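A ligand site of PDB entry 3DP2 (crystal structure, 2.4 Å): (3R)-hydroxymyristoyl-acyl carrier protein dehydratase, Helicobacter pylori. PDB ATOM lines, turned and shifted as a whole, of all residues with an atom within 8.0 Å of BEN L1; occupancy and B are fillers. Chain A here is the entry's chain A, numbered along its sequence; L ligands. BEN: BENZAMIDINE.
The side-chain amide nitrogen of Gln 40 lies close to a nitrogen (N2) of BEN L1 (2.8 Å).
A nitrogen (N1) of BEN L1 is in salt-bridge range of the side-chain carboxylate of Glu 124, 2.9 Å away.
N of Val 125 sits at hydrogen-bond distance from O of Gln 40, 2.8 Å away.
The backbone carbonyl oxygen of Gly 136 sits at hydrogen-bond distance from the backbone NH of Glu 124, at 2.8 Å.
Val 125 touches BEN L1.
Within 4 Å of BEN L1: Gln 40, Glu 124 and Val 125.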
ATOM      1  N   GLN A  37      -2.888  19.570 -10.253  1.00  0.00           N
ATOM      2  CA  GLN A  37      -4.189  19.950 -10.788  1.00  0.00           C
ATOM      3  C   GLN A  37      -5.110  18.753 -10.593  1.00  0.00           C
ATOM      4  O   GLN A  37      -4.949  17.724 -11.267  1.00  0.00           O
ATOM      5  CB  GLN A  37      -4.083  20.318 -12.264  1.00  0.00           C
ATOM      6  CG  GLN A  37      -5.415  20.746 -12.884  1.00  0.00           C
ATOM      7  CD  GLN A  37      -5.956  22.049 -12.315  1.00  0.00           C
ATOM      8  OE1 GLN A  37      -7.168  22.199 -12.089  1.00  0.00           O
ATOM      9  NE2 GLN A  37      -5.060  23.024 -12.096  1.00  0.00           N
ATOM     10  N   ALA A  38      -6.068  18.878  -9.683  1.00  0.00           N
ATOM     11  CA  ALA A  38      -7.026  17.826  -9.379  1.00  0.00           C
ATOM     12  C   ALA A  38      -7.599  17.110 -10.602  1.00  0.00           C
ATOM     13  O   ALA A  38      -8.042  17.751 -11.556  1.00  0.00           O
ATOM     14  CB  ALA A  38      -8.160  18.399  -8.549  1.00  0.00           C
ATOM     15  N   ASN A  39      -7.567  15.784 -10.536  1.00  0.00           N
ATOM     16  CA  ASN A  39      -8.086  14.913 -11.603  1.00  0.00           C
ATOM     17  C   ASN A  39      -7.396  15.048 -12.958  1.00  0.00           C
ATOM     18  O   ASN A  39      -7.830  14.428 -13.926  1.00  0.00           O
ATOM     19  CB  ASN A  39      -9.590  15.124 -11.798  1.00  0.00           C
ATOM     20  CG  ASN A  39     -10.359  15.029 -10.500  1.00  0.00           C
ATOM     21  OD1 ASN A  39     -10.910  16.023 -10.020  1.00  0.00           O
ATOM     22  ND2 ASN A  39     -10.406  13.836  -9.913  1.00  0.00           N
ATOM     23  N   GLN A  40      -6.338  15.839 -13.037  1.00  0.00           N
ATOM     24  CA  GLN A  40      -5.661  16.012 -14.307  1.00  0.00           C
ATOM     25  C   GLN A  40      -4.183  15.669 -14.332  1.00  0.00           C
ATOM     26  O   GLN A  40      -3.772  14.802 -15.099  1.00  0.00           O
ATOM     27  CB  GLN A  40      -5.837  17.444 -14.832  1.00  0.00           C
ATOM     28  CG  GLN A  40      -7.285  17.814 -15.082  1.00  0.00           C
ATOM     29  CD  GLN A  40      -7.423  19.093 -15.854  1.00  0.00           C
ATOM     30  OE1 GLN A  40      -8.122  20.011 -15.436  1.00  0.00           O
ATOM     31  NE2 GLN A  40      -6.752  19.179 -16.996  1.00  0.00           N
ATOM     32  N   LYS A  41      -3.383  16.321 -13.504  1.00  0.00           N
ATOM     33  CA  LYS A  41      -1.970  16.024 -13.509  1.00  0.00           C
ATOM     34  C   LYS A  41      -1.195  16.499 -12.310  1.00  0.00           C
ATOM     35  O   LYS A  41      -1.698  17.222 -11.440  1.00  0.00           O
ATOM     36  CB  LYS A  41      -1.321  16.631 -14.755  1.00  0.00           C
ATOM     37  CG  LYS A  41      -1.230  18.129 -14.700  1.00  0.00           C
ATOM     38  CD  LYS A  41      -0.128  18.614 -15.603  1.00  0.00           C
ATOM     39  CE  LYS A  41      -0.058  20.129 -15.578  1.00  0.00           C
ATOM     40  NZ  LYS A  41       0.943  20.614 -16.571  1.00  0.00           N
ATOM     41  N   ILE A  42       0.069  16.076 -12.271  1.00  0.00           N
ATOM     42  CA  ILE A  42       0.978  16.439 -11.214  1.00  0.00           C
ATOM     43  C   ILE A  42       2.400  16.474 -11.763  1.00  0.00           C
ATOM     44  O   ILE A  42       2.739  15.754 -12.705  1.00  0.00           O
ATOM     45  CB  ILE A  42       0.901  15.437 -10.027  1.00  0.00           C
ATOM     46  CG1 ILE A  42       1.843  15.882  -8.905  1.00  0.00           C
ATOM     47  CG2 ILE A  42       1.257  14.043 -10.493  1.00  0.00           C
ATOM     48  CD1 ILE A  42       1.681  15.090  -7.607  1.00  0.00           C
ATOM     49  N   LEU A 123       3.182  13.113 -14.389  1.00  0.00           N
ATOM     50  CA  LEU A 123       2.083  12.161 -14.523  1.00  0.00           C
ATOM     51  C   LEU A 123       0.791  12.880 -14.869  1.00  0.00           C
ATOM     52  O   LEU A 123       0.552  14.010 -14.446  1.00  0.00           O
ATOM     53  CB  LEU A 123       1.881  11.365 -13.225  1.00  0.00           C
ATOM     54  CG  LEU A 123       2.893  10.272 -12.830  1.00  0.00           C
ATOM     55  CD1 LEU A 123       2.889   9.168 -13.876  1.00  0.00           C
ATOM     56  CD2 LEU A 123       4.280  10.891 -12.684  1.00  0.00           C
ATOM     57  N   GLU A 124      -0.047  12.192 -15.624  1.00  0.00           N
ATOM     58  CA  GLU A 124      -1.328  12.740 -16.022  1.00  0.00           C
ATOM     59  C   GLU A 124      -2.394  11.654 -15.920  1.00  0.00           C
ATOM     60  O   GLU A 124      -2.111  10.471 -16.133  1.00  0.00           O
ATOM     61  CB  GLU A 124      -1.206  13.342 -17.429  1.00  0.00           C
ATOM     62  CG  GLU A 124      -0.087  14.408 -17.460  1.00  0.00           C
ATOM     63  CD  GLU A 124      -0.180  15.373 -18.605  1.00  0.00           C
ATOM     64  OE1 GLU A 124       0.118  14.975 -19.764  1.00  0.00           O
ATOM     65  OE2 GLU A 124      -0.557  16.543 -18.359  1.00  0.00           O
ATOM     66  N   VAL A 125      -3.608  12.061 -15.558  1.00  0.00           N
ATOM     67  CA  VAL A 125      -4.729  11.132 -15.407  1.00  0.00           C
ATOM     68  C   VAL A 125      -5.362  10.719 -16.737  1.00  0.00           C
ATOM     69  O   VAL A 125      -5.947  11.539 -17.450  1.00  0.00           O
ATOM     70  CB  VAL A 125      -5.820  11.758 -14.508  1.00  0.00           C
ATOM     71  CG1 VAL A 125      -6.959  10.753 -14.294  1.00  0.00           C
ATOM     72  CG2 VAL A 125      -5.214  12.196 -13.185  1.00  0.00           C
ATOM     73  N   LEU A 126      -5.235   9.433 -17.064  1.00  0.00           N
ATOM     74  CA  LEU A 126      -5.778   8.912 -18.303  1.00  0.00           C
ATOM     75  C   LEU A 126      -7.213   8.446 -18.100  1.00  0.00           C
ATOM     76  O   LEU A 126      -8.031   8.524 -19.022  1.00  0.00           O
ATOM     77  CB  LEU A 126      -4.913   7.763 -18.807  1.00  0.00           C
ATOM     78  CG  LEU A 126      -3.403   8.062 -18.889  1.00  0.00           C
ATOM     79  CD1 LEU A 126      -2.654   6.807 -19.266  1.00  0.00           C
ATOM     80  CD2 LEU A 126      -3.152   9.168 -19.909  1.00  0.00           C
ATOM     81  N   LYS A 127      -7.533   7.985 -16.893  1.00  0.00           N
ATOM     82  CA  LYS A 127      -8.879   7.514 -16.565  1.00  0.00           C
ATOM     83  C   LYS A 127      -9.039   7.320 -15.060  1.00  0.00           C
ATOM     84  O   LYS A 127      -8.149   6.813 -14.380  1.00  0.00           O
ATOM     85  CB  LYS A 127      -9.148   6.192 -17.284  1.00  0.00           C
ATOM     86  CG  LYS A 127     -10.563   5.631 -17.095  1.00  0.00           C
ATOM     87  CD  LYS A 127     -10.759   4.370 -17.950  1.00  0.00           C
ATOM     88  CE  LYS A 127     -12.226   3.972 -18.076  1.00  0.00           C
ATOM     89  NZ  LYS A 127     -12.773   3.457 -16.795  1.00  0.00           N
ATOM     90  N   GLN A 134      -5.934   5.475 -13.413  1.00  0.00           N
ATOM     91  CA  GLN A 134      -4.985   5.181 -14.480  1.00  0.00           C
ATOM     92  C   GLN A 134      -4.205   6.433 -14.815  1.00  0.00           C
ATOM     93  O   GLN A 134      -4.783   7.429 -15.230  1.00  0.00           O
ATOM     94  CB  GLN A 134      -5.702   4.707 -15.735  1.00  0.00           C
ATOM     95  CG  GLN A 134      -5.864   3.217 -15.830  1.00  0.00           C
ATOM     96  CD  GLN A 134      -6.631   2.837 -17.062  1.00  0.00           C
ATOM     97  OE1 GLN A 134      -6.317   3.288 -18.177  1.00  0.00           O
ATOM     98  NE2 GLN A 134      -7.653   2.007 -16.896  1.00  0.00           N
ATOM     99  N   GLY A 136      -0.350   8.109 -16.527  1.00  0.00           N
ATOM    100  CA  GLY A 136       0.713   7.839 -17.445  1.00  0.00           C
ATOM    101  C   GLY A 136       1.536   9.097 -17.537  1.00  0.00           C
ATOM    102  O   GLY A 136       1.025  10.196 -17.307  1.00  0.00           O
HETATM  103  C1  BEN L   1      -4.078  15.419 -19.239  1.00  0.00           C
HETATM  104  C2  BEN L   1      -4.970  14.344 -19.169  1.00  0.00           C
HETATM  105  C3  BEN L   1      -4.795  13.233 -19.980  1.00  0.00           C
HETATM  106  C4  BEN L   1      -3.724  13.187 -20.869  1.00  0.00           C
HETATM  107  C5  BEN L   1      -2.830  14.249 -20.934  1.00  0.00           C
HETATM  108  C6  BEN L   1      -3.005  15.360 -20.123  1.00  0.00           C
HETATM  109  C   BEN L   1      -4.292  16.558 -18.466  1.00  0.00           C
HETATM  110  N1  BEN L   1      -3.288  17.383 -18.205  1.00  0.00           N
HETATM  111  N2  BEN L   1      -5.517  16.838 -18.035  1.00  0.00           N
HETATM  112  C1  BEN L   2       4.047  10.164 -22.847  1.00  0.00           C
HETATM  113  C2  BEN L   2       4.280   8.844 -23.307  1.00  0.00           C
HETATM  114  C3  BEN L   2       5.400   8.546 -24.132  1.00  0.00           C
HETATM  115  C4  BEN L   2       6.289   9.570 -24.512  1.00  0.00           C
HETATM  116  C5  BEN L   2       6.075  10.895 -24.062  1.00  0.00           C
HETATM  117  C6  BEN L   2       4.952  11.185 -23.239  1.00  0.00           C
HETATM  118  C   BEN L   2       2.963  10.461 -21.993  1.00  0.00           C
HETATM  119  N1  BEN L   2       2.783  11.712 -21.529  1.00  0.00           N
HETATM  120  N2  BEN L   2       2.119   9.489 -21.588  1.00  0.00           N
